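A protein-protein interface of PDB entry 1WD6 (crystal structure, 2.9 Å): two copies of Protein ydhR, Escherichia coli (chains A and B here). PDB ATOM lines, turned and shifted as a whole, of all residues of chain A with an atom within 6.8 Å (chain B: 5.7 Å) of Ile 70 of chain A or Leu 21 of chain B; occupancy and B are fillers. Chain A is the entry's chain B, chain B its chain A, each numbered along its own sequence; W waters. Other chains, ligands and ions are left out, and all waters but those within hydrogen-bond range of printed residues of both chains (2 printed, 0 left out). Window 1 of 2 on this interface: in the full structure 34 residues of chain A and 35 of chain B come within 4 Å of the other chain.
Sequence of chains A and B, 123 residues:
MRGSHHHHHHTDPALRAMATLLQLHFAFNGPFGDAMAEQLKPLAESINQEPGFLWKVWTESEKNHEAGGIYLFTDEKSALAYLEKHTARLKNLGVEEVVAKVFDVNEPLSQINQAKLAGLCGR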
ATOM      1  N   LEU A  21       7.052 -31.656 -12.498  1.00  0.00           N
ATOM      2  CA  LEU A  21       5.864 -31.494 -11.678  1.00  0.00           C
ATOM      3  C   LEU A  21       5.143 -32.826 -11.562  1.00  0.00           C
ATOM      4  O   LEU A  21       4.768 -33.427 -12.564  1.00  0.00           O
ATOM      5  CB  LEU A  21       4.911 -30.443 -12.270  1.00  0.00           C
ATOM      6  CG  LEU A  21       3.542 -30.285 -11.583  1.00  0.00           C
ATOM      7  CD1 LEU A  21       3.117 -28.831 -11.587  1.00  0.00           C
ATOM      8  CD2 LEU A  21       2.510 -31.156 -12.276  1.00  0.00           C
ATOM      9  N   LEU A  22       4.969 -33.287 -10.331  1.00  0.00           N
ATOM     10  CA  LEU A  22       4.274 -34.536 -10.066  1.00  0.00           C
ATOM     11  C   LEU A  22       2.838 -34.173  -9.715  1.00  0.00           C
ATOM     12  O   LEU A  22       2.602 -33.351  -8.833  1.00  0.00           O
ATOM     13  CB  LEU A  22       4.911 -35.250  -8.871  1.00  0.00           C
ATOM     14  CG  LEU A  22       4.592 -36.716  -8.565  1.00  0.00           C
ATOM     15  CD1 LEU A  22       4.496 -36.870  -7.057  1.00  0.00           C
ATOM     16  CD2 LEU A  22       3.306 -37.158  -9.218  1.00  0.00           C
ATOM     17  N   GLN A  23       1.878 -34.766 -10.408  1.00  0.00           N
ATOM     18  CA  GLN A  23       0.486 -34.493 -10.103  1.00  0.00           C
ATOM     19  C   GLN A  23      -0.213 -35.830  -9.878  1.00  0.00           C
ATOM     20  O   GLN A  23      -0.197 -36.701 -10.749  1.00  0.00           O
ATOM     21  CB  GLN A  23      -0.175 -33.711 -11.251  1.00  0.00           C
ATOM     22  CG  GLN A  23      -0.660 -34.543 -12.434  1.00  0.00           C
ATOM     23  CD  GLN A  23      -1.411 -33.719 -13.472  1.00  0.00           C
ATOM     24  OE1 GLN A  23      -2.244 -34.243 -14.217  1.00  0.00           O
ATOM     25  NE2 GLN A  23      -1.110 -32.428 -13.534  1.00  0.00           N
ATOM     26  N   LEU A  24      -0.793 -36.020  -8.702  1.00  0.00           N
ATOM     27  CA  LEU A  24      -1.487 -37.275  -8.446  1.00  0.00           C
ATOM     28  C   LEU A  24      -2.672 -37.094  -7.514  1.00  0.00           C
ATOM     29  O   LEU A  24      -2.722 -36.145  -6.726  1.00  0.00           O
ATOM     30  CB  LEU A  24      -0.543 -38.323  -7.845  1.00  0.00           C
ATOM     31  CG  LEU A  24      -0.216 -38.203  -6.352  1.00  0.00           C
ATOM     32  CD1 LEU A  24       0.006 -39.574  -5.777  1.00  0.00           C
ATOM     33  CD2 LEU A  24       1.008 -37.342  -6.147  1.00  0.00           C
ATOM     34  N   PHE A  53      12.624 -31.860  -3.373  1.00  0.00           N
ATOM     35  CA  PHE A  53      11.291 -31.322  -3.148  1.00  0.00           C
ATOM     36  C   PHE A  53      11.341 -29.805  -3.089  1.00  0.00           C
ATOM     37  O   PHE A  53      12.191 -29.242  -2.399  1.00  0.00           O
ATOM     38  CB  PHE A  53      10.725 -31.849  -1.836  1.00  0.00           C
ATOM     39  CG  PHE A  53       9.376 -31.305  -1.513  1.00  0.00           C
ATOM     40  CD1 PHE A  53       8.267 -31.700  -2.239  1.00  0.00           C
ATOM     41  CD2 PHE A  53       9.217 -30.356  -0.519  1.00  0.00           C
ATOM     42  CE1 PHE A  53       7.015 -31.152  -1.979  1.00  0.00           C
ATOM     43  CE2 PHE A  53       7.975 -29.802  -0.252  1.00  0.00           C
ATOM     44  CZ  PHE A  53       6.873 -30.199  -0.983  1.00  0.00           C
ATOM     45  N   TRP A  55       7.968 -27.603  -3.602  1.00  0.00           N
ATOM     46  CA  TRP A  55       6.714 -27.237  -2.950  1.00  0.00           C
ATOM     47  C   TRP A  55       5.549 -28.129  -3.367  1.00  0.00           C
ATOM     48  O   TRP A  55       5.558 -28.732  -4.448  1.00  0.00           O
ATOM     49  CB  TRP A  55       6.356 -25.768  -3.192  1.00  0.00           C
ATOM     50  CG  TRP A  55       6.253 -25.393  -4.609  1.00  0.00           C
ATOM     51  CD1 TRP A  55       7.221 -24.818  -5.373  1.00  0.00           C
ATOM     52  CD2 TRP A  55       5.131 -25.608  -5.470  1.00  0.00           C
ATOM     53  NE1 TRP A  55       6.775 -24.662  -6.663  1.00  0.00           N
ATOM     54  CE2 TRP A  55       5.494 -25.141  -6.752  1.00  0.00           C
ATOM     55  CE3 TRP A  55       3.854 -26.157  -5.286  1.00  0.00           C
ATOM     56  CZ2 TRP A  55       4.627 -25.206  -7.846  1.00  0.00           C
ATOM     57  CZ3 TRP A  55       2.992 -26.222  -6.377  1.00  0.00           C
ATOM     58  CH2 TRP A  55       3.384 -25.749  -7.639  1.00  0.00           C
ATOM     59  N   LYS A  56       4.554 -28.219  -2.488  1.00  0.00           N
ATOM     60  CA  LYS A  56       3.378 -29.035  -2.735  1.00  0.00           C
ATOM     61  C   LYS A  56       2.121 -28.278  -2.388  1.00  0.00           C
ATOM     62  O   LYS A  56       2.092 -27.525  -1.415  1.00  0.00           O
ATOM     63  CB  LYS A  56       3.418 -30.302  -1.883  1.00  0.00           C
ATOM     64  CG  LYS A  56       2.144 -31.138  -1.965  1.00  0.00           C
ATOM     65  CD  LYS A  56       2.110 -32.240  -0.905  1.00  0.00           C
ATOM     66  CE  LYS A  56       0.906 -33.151  -1.092  1.00  0.00           C
ATOM     67  NZ  LYS A  56       0.871 -34.264  -0.111  1.00  0.00           N
ATOM     68  N   VAL A  57       1.089 -28.472  -3.200  1.00  0.00           N
ATOM     69  CA  VAL A  57      -0.209 -27.864  -2.957  1.00  0.00           C
ATOM     70  C   VAL A  57      -1.115 -29.061  -2.682  1.00  0.00           C
ATOM     71  O   VAL A  57      -1.261 -29.948  -3.532  1.00  0.00           O
ATOM     72  CB  VAL A  57      -0.748 -27.107  -4.189  1.00  0.00           C
ATOM     73  CG1 VAL A  57      -2.179 -26.671  -3.939  1.00  0.00           C
ATOM     74  CG2 VAL A  57       0.106 -25.893  -4.473  1.00  0.00           C
ATOM     75  N   TRP A  58      -1.703 -29.099  -1.491  1.00  0.00           N
ATOM     76  CA  TRP A  58      -2.570 -30.204  -1.122  1.00  0.00           C
ATOM     77  C   TRP A  58      -3.930 -30.088  -1.766  1.00  0.00           C
ATOM     78  O   TRP A  58      -4.607 -29.062  -1.669  1.00  0.00           O
ATOM     79  CB  TRP A  58      -2.694 -30.296   0.386  1.00  0.00           C
ATOM     80  CG  TRP A  58      -1.440 -30.771   1.017  1.00  0.00           C
ATOM     81  CD1 TRP A  58      -0.270 -30.080   1.153  1.00  0.00           C
ATOM     82  CD2 TRP A  58      -1.214 -32.059   1.577  1.00  0.00           C
ATOM     83  NE1 TRP A  58       0.674 -30.863   1.766  1.00  0.00           N
ATOM     84  CE2 TRP A  58       0.119 -32.085   2.039  1.00  0.00           C
ATOM     85  CE3 TRP A  58      -2.010 -33.202   1.735  1.00  0.00           C
ATOM     86  CZ2 TRP A  58       0.673 -33.208   2.649  1.00  0.00           C
ATOM     87  CZ3 TRP A  58      -1.461 -34.314   2.334  1.00  0.00           C
ATOM     88  CH2 TRP A  58      -0.131 -34.311   2.786  1.00  0.00           C
ATOM     89  N   THR A  59      -4.313 -31.181  -2.413  1.00  0.00           N
ATOM     90  CA  THR A  59      -5.551 -31.304  -3.163  1.00  0.00           C
ATOM     91  C   THR A  59      -6.605 -32.146  -2.444  1.00  0.00           C
ATOM     92  O   THR A  59      -6.289 -33.200  -1.903  1.00  0.00           O
ATOM     93  CB  THR A  59      -5.199 -31.935  -4.519  1.00  0.00           C
ATOM     94  OG1 THR A  59      -4.912 -30.899  -5.460  1.00  0.00           O
ATOM     95  CG2 THR A  59      -6.292 -32.835  -5.016  1.00  0.00           C
ATOM     96  N   GLY A  68      -5.346 -35.511  -3.188  1.00  0.00           N
ATOM     97  CA  GLY A  68      -4.118 -35.689  -3.934  1.00  0.00           C
ATOM     98  C   GLY A  68      -3.126 -34.578  -3.699  1.00  0.00           C
ATOM     99  O   GLY A  68      -2.979 -34.083  -2.583  1.00  0.00           O
ATOM    100  N   GLY A  69      -2.425 -34.185  -4.751  1.00  0.00           N
ATOM    101  CA  GLY A  69      -1.460 -33.124  -4.586  1.00  0.00           C
ATOM    102  C   GLY A  69      -0.653 -32.829  -5.823  1.00  0.00           C
ATOM    103  O   GLY A  69      -0.500 -33.677  -6.704  1.00  0.00           O
ATOM    104  N   ILE A  70      -0.147 -31.605  -5.878  1.00  0.00           N
ATOM    105  CA  ILE A  70       0.674 -31.146  -6.982  1.00  0.00           C
ATOM    106  C   ILE A  70       2.051 -30.904  -6.375  1.00  0.00           C
ATOM    107  O   ILE A  70       2.235 -29.973  -5.586  1.00  0.00           O
ATOM    108  CB  ILE A  70       0.115 -29.816  -7.573  1.00  0.00           C
ATOM    109  CG1 ILE A  70      -1.336 -30.016  -8.032  1.00  0.00           C
ATOM    110  CG2 ILE A  70       0.988 -29.331  -8.714  1.00  0.00           C
ATOM    111  CD1 ILE A  70      -1.548 -31.186  -8.987  1.00  0.00           C
ATOM    112  N   TYR A  71       3.013 -31.755  -6.714  1.00  0.00           N
ATOM    113  CA  TYR A  71       4.358 -31.601  -6.184  1.00  0.00           C
ATOM    114  C   TYR A  71       5.253 -30.983  -7.230  1.00  0.00           C
ATOM    115  O   TYR A  71       5.002 -31.110  -8.415  1.00  0.00           O
ATOM    116  CB  TYR A  71       4.969 -32.951  -5.797  1.00  0.00           C
ATOM    117  CG  TYR A  71       4.257 -33.712  -4.710  1.00  0.00           C
ATOM    118  CD1 TYR A  71       3.048 -34.361  -4.962  1.00  0.00           C
ATOM    119  CD2 TYR A  71       4.819 -33.838  -3.441  1.00  0.00           C
ATOM    120  CE1 TYR A  71       2.421 -35.124  -3.980  1.00  0.00           C
ATOM    121  CE2 TYR A  71       4.196 -34.605  -2.447  1.00  0.00           C
ATOM    122  CZ  TYR A  71       2.998 -35.248  -2.724  1.00  0.00           C
ATOM    123  OH  TYR A  71       2.387 -36.035  -1.762  1.00  0.00           O
ATOM    124  N   LEU A  72       6.302 -30.304  -6.791  1.00  0.00           N
ATOM    125  CA  LEU A  72       7.250 -29.734  -7.729  1.00  0.00           C
ATOM    126  C   LEU A  72       8.640 -30.123  -7.253  1.00  0.00           C
ATOM    127  O   LEU A  72       9.059 -29.745  -6.147  1.00  0.00           O
ATOM    128  CB  LEU A  72       7.136 -28.206  -7.806  1.00  0.00           C
ATOM    129  CG  LEU A  72       7.692 -27.781  -9.170  1.00  0.00           C
ATOM    130  CD1 LEU A  72       6.520 -27.585 -10.102  1.00  0.00           C
ATOM    131  CD2 LEU A  72       8.533 -26.536  -9.086  1.00  0.00           C
ATOM    132  N   ALA B  19      -9.527 -21.568  -1.983  1.00  0.00           N
ATOM    133  CA  ALA B  19      -9.113 -21.508  -3.422  1.00  0.00           C
ATOM    134  C   ALA B  19      -9.318 -22.832  -4.156  1.00  0.00           C
ATOM    135  O   ALA B  19      -9.164 -23.908  -3.582  1.00  0.00           O
ATOM    136  CB  ALA B  19      -7.654 -21.092  -3.525  1.00  0.00           C
ATOM    137  N   THR B  20      -9.659 -22.746  -5.434  1.00  0.00           N
ATOM    138  CA  THR B  20      -9.879 -23.937  -6.242  1.00  0.00           C
ATOM    139  C   THR B  20      -8.661 -24.211  -7.116  1.00  0.00           C
ATOM    140  O   THR B  20      -7.959 -23.287  -7.525  1.00  0.00           O
ATOM    141  CB  THR B  20     -11.118 -23.761  -7.149  1.00  0.00           C
ATOM    142  OG1 THR B  20     -12.301 -23.765  -6.340  1.00  0.00           O
ATOM    143  CG2 THR B  20     -11.198 -24.872  -8.183  1.00  0.00           C
ATOM    144  N   LEU B  21      -8.401 -25.484  -7.393  1.00  0.00           N
ATOM    145  CA  LEU B  21      -7.275 -25.849  -8.236  1.00  0.00           C
ATOM    146  C   LEU B  21      -7.744 -26.634  -9.452  1.00  0.00           C
ATOM    147  O   LEU B  21      -8.397 -27.671  -9.334  1.00  0.00           O
ATOM    148  CB  LEU B  21      -6.241 -26.668  -7.450  1.00  0.00           C
ATOM    149  CG  LEU B  21      -5.062 -27.190  -8.285  1.00  0.00           C
ATOM    150  CD1 LEU B  21      -3.757 -26.961  -7.559  1.00  0.00           C
ATOM    151  CD2 LEU B  21      -5.263 -28.667  -8.589  1.00  0.00           C
ATOM    152  N   LEU B  22      -7.422 -26.112 -10.626  1.00  0.00           N
ATOM    153  CA  LEU B  22      -7.779 -26.768 -11.872  1.00  0.00           C
ATOM    154  C   LEU B  22      -6.536 -27.526 -12.311  1.00  0.00           C
ATOM    155  O   LEU B  22      -5.479 -26.937 -12.527  1.00  0.00           O
ATOM    156  CB  LEU B  22      -8.175 -25.732 -12.921  1.00  0.00           C
ATOM    157  CG  LEU B  22      -8.532 -26.261 -14.306  1.00  0.00           C
ATOM    158  CD1 LEU B  22      -9.689 -27.235 -14.205  1.00  0.00           C
ATOM    159  CD2 LEU B  22      -8.892 -25.094 -15.203  1.00  0.00           C
ATOM    160  N   GLN B  23      -6.663 -28.841 -12.409  1.00  0.00           N
ATOM    161  CA  GLN B  23      -5.560 -29.703 -12.804  1.00  0.00           C
ATOM    162  C   GLN B  23      -5.927 -30.301 -14.137  1.00  0.00           C
ATOM    163  O   GLN B  23      -6.886 -31.063 -14.224  1.00  0.00           O
ATOM    164  CB  GLN B  23      -5.397 -30.809 -11.772  1.00  0.00           C
ATOM    165  CG  GLN B  23      -4.699 -32.047 -12.269  1.00  0.00           C
ATOM    166  CD  GLN B  23      -4.921 -33.221 -11.339  1.00  0.00           C
ATOM    167  OE1 GLN B  23      -4.560 -33.173 -10.161  1.00  0.00           O
ATOM    168  NE2 GLN B  23      -5.527 -34.282 -11.862  1.00  0.00           N
ATOM    169  N   TRP B  55      -2.490 -18.108 -10.600  1.00  0.00           N
ATOM    170  CA  TRP B  55      -1.229 -18.538 -11.203  1.00  0.00           C
ATOM    171  C   TRP B  55      -1.426 -19.823 -11.984  1.00  0.00           C
ATOM    172  O   TRP B  55      -2.488 -20.455 -11.925  1.00  0.00           O
ATOM    173  CB  TRP B  55      -0.097 -18.718 -10.170  1.00  0.00           C
ATOM    174  CG  TRP B  55      -0.363 -19.637  -8.998  1.00  0.00           C
ATOM    175  CD1 TRP B  55      -0.802 -19.269  -7.760  1.00  0.00           C
ATOM    176  CD2 TRP B  55      -0.202 -21.069  -8.955  1.00  0.00           C
ATOM    177  NE1 TRP B  55      -0.924 -20.374  -6.948  1.00  0.00           N
ATOM    178  CE2 TRP B  55      -0.565 -21.491  -7.655  1.00  0.00           C
ATOM    179  CE3 TRP B  55       0.207 -22.034  -9.887  1.00  0.00           C
ATOM    180  CZ2 TRP B  55      -0.530 -22.840  -7.263  1.00  0.00           C
ATOM    181  CZ3 TRP B  55       0.239 -23.380  -9.493  1.00  0.00           C
ATOM    182  CH2 TRP B  55      -0.128 -23.764  -8.193  1.00  0.00           C
ATOM    183  N   ILE B  70      -1.527 -26.462 -14.412  1.00  0.00           N
ATOM    184  CA  ILE B  70      -2.081 -26.472 -13.069  1.00  0.00           C
ATOM    185  C   ILE B  70      -2.467 -25.017 -12.785  1.00  0.00           C
ATOM    186  O   ILE B  70      -1.597 -24.147 -12.698  1.00  0.00           O
ATOM    187  CB  ILE B  70      -1.022 -26.946 -12.026  1.00  0.00           C
ATOM    188  CG1 ILE B  70      -0.495 -28.341 -12.402  1.00  0.00           C
ATOM    189  CG2 ILE B  70      -1.623 -26.919 -10.614  1.00  0.00           C
ATOM    190  CD1 ILE B  70      -1.564 -29.420 -12.459  1.00  0.00           C
ATOM    191  N   TYR B  71      -3.763 -24.747 -12.672  1.00  0.00           N
ATOM    192  CA  TYR B  71      -4.218 -23.387 -12.411  1.00  0.00           C
ATOM    193  C   TYR B  71      -4.806 -23.274 -11.023  1.00  0.00           C
ATOM    194  O   TYR B  71      -5.388 -24.223 -10.511  1.00  0.00           O
ATOM    195  CB  TYR B  71      -5.309 -22.959 -13.396  1.00  0.00           C
ATOM    196  CG  TYR B  71      -4.979 -23.067 -14.862  1.00  0.00           C
ATOM    197  CD1 TYR B  71      -4.756 -24.311 -15.454  1.00  0.00           C
ATOM    198  CD2 TYR B  71      -4.971 -21.934 -15.676  1.00  0.00           C
ATOM    199  CE1 TYR B  71      -4.538 -24.427 -16.831  1.00  0.00           C
ATOM    200  CE2 TYR B  71      -4.756 -22.034 -17.056  1.00  0.00           C
ATOM    201  CZ  TYR B  71      -4.542 -23.286 -17.629  1.00  0.00           C
ATOM    202  OH  TYR B  71      -4.343 -23.408 -18.991  1.00  0.00           O
ATOM    203  N   LEU B  72      -4.670 -22.101 -10.422  1.00  0.00           N
ATOM    204  CA  LEU B  72      -5.235 -21.867  -9.105  1.00  0.00           C
ATOM    205  C   LEU B  72      -6.130 -20.631  -9.180  1.00  0.00           C
ATOM    206  O   LEU B  72      -5.652 -19.515  -9.370  1.00  0.00           O
ATOM    207  CB  LEU B  72      -4.131 -21.650  -8.073  1.00  0.00           C
ATOM    208  CG  LEU B  72      -4.673 -21.537  -6.647  1.00  0.00           C
ATOM    209  CD1 LEU B  72      -5.287 -22.861  -6.237  1.00  0.00           C
ATOM    210  CD2 LEU B  72      -3.561 -21.165  -5.698  1.00  0.00           C
ATOM    211  N   PHE B  73      -7.435 -20.835  -9.052  1.00  0.00           N
ATOM    212  CA  PHE B  73      -8.375 -19.729  -9.109  1.00  0.00           C
ATOM    213  C   PHE B  73      -8.877 -19.382  -7.729  1.00  0.00           C
ATOM    214  O   PHE B  73      -8.705 -20.150  -6.787  1.00  0.00           O
ATOM    215  CB  PHE B  73      -9.560 -20.078  -9.999  1.00  0.00           C
ATOM    216  CG  PHE B  73      -9.218 -20.155 -11.451  1.00  0.00           C
ATOM    217  CD1 PHE B  73      -8.597 -21.287 -11.974  1.00  0.00           C
ATOM    218  CD2 PHE B  73      -9.496 -19.088 -12.298  1.00  0.00           C
ATOM    219  CE1 PHE B  73      -8.261 -21.351 -13.318  1.00  0.00           C
ATOM    220  CE2 PHE B  73      -9.164 -19.142 -13.640  1.00  0.00           C
ATOM    221  CZ  PHE B  73      -8.546 -20.273 -14.153  1.00  0.00           C
ATOM    222  N   LYS B 101      -9.717 -31.978 -13.699  1.00  0.00           N
ATOM    223  CA  LYS B 101     -10.115 -32.252 -12.327  1.00  0.00           C
ATOM    224  C   LYS B 101     -10.160 -30.954 -11.540  1.00  0.00           C
ATOM    225  O   LYS B 101      -9.245 -30.136 -11.636  1.00  0.00           O
ATOM    226  CB  LYS B 101      -9.124 -33.212 -11.676  1.00  0.00           C
ATOM    227  CG  LYS B 101      -9.444 -34.674 -11.923  1.00  0.00           C
ATOM    228  CD  LYS B 101      -9.929 -35.337 -10.644  1.00  0.00           C
ATOM    229  CE  LYS B 101     -10.586 -36.674 -10.910  1.00  0.00           C
ATOM    230  NZ  LYS B 101     -11.871 -36.493 -11.641  1.00  0.00           N
ATOM    231  N   VAL B 102     -11.230 -30.754 -10.775  1.00  0.00           N
ATOM    232  CA  VAL B 102     -11.356 -29.548  -9.963  1.00  0.00           C
ATOM    233  C   VAL B 102     -11.254 -29.936  -8.496  1.00  0.00           C
ATOM    234  O   VAL B 102     -12.043 -30.731  -7.984  1.00  0.00           O
ATOM    235  CB  VAL B 102     -12.699 -28.833 -10.198  1.00  0.00           C
ATOM    236  CG1 VAL B 102     -12.743 -27.538  -9.404  1.00  0.00           C
ATOM    237  CG2 VAL B 102     -12.875 -28.545 -11.665  1.00  0.00           C
ATOM    238  N   PHE B 103     -10.276 -29.365  -7.817  1.00  0.00           N
ATOM    239  CA  PHE B 103     -10.064 -29.688  -6.423  1.00  0.00           C
ATOM    240  C   PHE B 103     -10.070 -28.466  -5.540  1.00  0.00           C
ATOM    241  O   PHE B 103      -9.909 -27.346  -6.013  1.00  0.00           O
ATOM    242  CB  PHE B 103      -8.714 -30.393  -6.248  1.00  0.00           C
ATOM    243  CG  PHE B 103      -8.646 -31.760  -6.868  1.00  0.00           C
ATOM    244  CD1 PHE B 103      -7.649 -32.070  -7.789  1.00  0.00           C
ATOM    245  CD2 PHE B 103      -9.542 -32.755  -6.494  1.00  0.00           C
ATOM    246  CE1 PHE B 103      -7.541 -33.349  -8.325  1.00  0.00           C
ATOM    247  CE2 PHE B 103      -9.442 -34.038  -7.025  1.00  0.00           C
ATOM    248  CZ  PHE B 103      -8.436 -34.334  -7.943  1.00  0.00           C
ATOM    249  N   ASP B 104     -10.272 -28.699  -4.249  1.00  0.00           N
ATOM    250  CA  ASP B 104     -10.222 -27.634  -3.266  1.00  0.00           C
ATOM    251  C   ASP B 104      -8.822 -27.792  -2.705  1.00  0.00           C
ATOM    252  O   ASP B 104      -8.250 -28.883  -2.744  1.00  0.00           O
ATOM    253  CB  ASP B 104     -11.239 -27.850  -2.146  1.00  0.00           C
ATOM    254  CG  ASP B 104     -12.668 -27.700  -2.615  1.00  0.00           C
ATOM    255  OD1 ASP B 104     -13.006 -26.631  -3.174  1.00  0.00           O
ATOM    256  OD2 ASP B 104     -13.456 -28.652  -2.418  1.00  0.00           O
ATOM    257  N   VAL B 105      -8.258 -26.717  -2.192  1.00  0.00           N
ATOM    258  CA  VAL B 105      -6.924 -26.797  -1.643  1.00  0.00           C
ATOM    259  C   VAL B 105      -6.971 -26.793  -0.127  1.00  0.00           C
ATOM    260  O   VAL B 105      -7.739 -26.043   0.476  1.00  0.00           O
ATOM    261  CB  VAL B 105      -6.075 -25.611  -2.093  1.00  0.00           C
ATOM    262  CG1 VAL B 105      -4.657 -25.778  -1.580  1.00  0.00           C
ATOM    263  CG2 VAL B 105      -6.114 -25.492  -3.605  1.00  0.00           C
HETATM  264  O   HOH W   1      -4.275 -33.398  -7.561  1.00  0.00           O
HETATM  265  O   HOH W   2      -5.126 -33.626 -15.228  1.00  0.00           O
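The backbone NH (N) of Val 57 of chain A sits at hydrogen-bond distance from the backbone carbonyl oxygen (O) of Ile 70 of chain A (3.0 Å).
The backbone carbonyl oxygen (O) of Thr 59 of chain A is in hydrogen-bond range of the backbone NH (N) of Gly 68 of chain A (2.8 Å).
The backbone carbonyl oxygen of Ala 19 of chain B sits at hydrogen-bond distance from the backbone NH of Val 105 of chain B, 3.3 Å away.
The backbone NH (N) of Gln 23 of chain B is in hydrogen-bond range of the backbone carbonyl oxygen (O) of Lys 101 of chain B (3.0 Å).
O of Phe 103 of chain B sits at hydrogen-bond distance from N of Leu 21 of chain B.
Among the printed residues, pairs that only touch across the chains: Leu 21 of chain A with Ile 70 of chain B (3.7 Å), Gln 23 of chain A with Gln 23 of chain B (3.8 Å), Gln 23 of chain A with Ile 70 of chain B (3.2 Å), Val 57 of chain A with Leu 21 of chain B (3.96 Å), Val 57 of chain A with Val 105 of chain B (3.5 Å), Trp 58 of chain A with Asp 104 of chain B (3.8 Å), Trp 58 of chain A with Val 105 of chain B (3.2 Å), Thr 59 of chain A with Leu 21 of chain B (3.9 Å), Thr 59 of chain A with Phe 103 of chain B (3.2 Å), Thr 59 of chain A with Asp 104 of chain B (3.6 Å), Ile 70 of chain A with Leu 21 of chain B (3.9 Å), Ile 70 of chain A with Gln 23 of chain B (3.8 Å) and Ile 70 of chain A with Ile 70 of chain B (3.9 Å).
Of the printed residues of chain B, Gln 23 of chain A touches Gln 23 (3.8 Å) and Ile 70 (3.2 Å).
Leu 24 of chain A touches none of the printed residues of chain B.
Printed residues of chain B within 4 Å of Trp 58 of chain A: Asp 104 and Val 105.
Of the printed residues of chain B, Ile 70 of chain A touches Leu 21 (3.9 Å), Gln 23 (3.8 Å) and Ile 70 (3.9 Å).
Of the printed residues of chain A, Leu 21 of chain B touches Val 57, Thr 59 and Ile 70.
Of the printed residues of chain A, Val 105 of chain B touches Val 57 (3.5 Å) and Trp 58 (3.2 Å).
The nearest printed residue of chain B that does not touch Ile 70 of chain A is Trp 55 of chain B (5.7 Å).
Of the 15 printed residues of chain B, 6 touch a printed residue of chain A.
Hydrophobic or aromatic side chains of chain B within 4 Å of the printed part of chain A: Leu 21, Ile 70, Phe 103 and Val 105.
Along chain B the printed residues that touch a printed residue of chain A span positions 21 to 105.
Hydrophobic or aromatic side chains of chain A within 4 Å of the printed part of chain B: Leu 21, Val 57 and Ile 70.
Among the printed residues, 13 pairs touch across the chains.
Among the printed residues, no Asp or Glu carboxylate lies within 4 Å of a Lys or Arg side-chain nitrogen of the other chain.
Leu 21 of chain A touches Ile 70 of chain B, and with the chains exchanged Ile 70 of chain A touches Leu 21 of chain B.
Gln 23 of chain B touches its own counterpart, Gln 23 of chain A.
Gln 23 of chain A touches Ile 70 of chain B, and with the chains exchanged Ile 70 of chain A touches Gln 23 of chain B.
Ile 70 of chain B touches its own counterpart, Ile 70 of chain A.
7 positions are printed for both chains.
Of the 13 pairs that touch across the chains among the printed residues, 6 have their exchanged pair printed and touching as well.
Water W1 lies within hydrogen-bond range of OE1 of Gln 23 of chain B (2.6 Å), O of Leu 24 of chain A (3.3 Å), OG1 of Thr 59 of chain A (3.3 Å) and N of Gly 69 of chain A (3.5 Å).
Water W2 bridges OE1 of Gln 23 of chain A (3.1 Å) and O of Gln 23 of chain B (3.3 Å).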
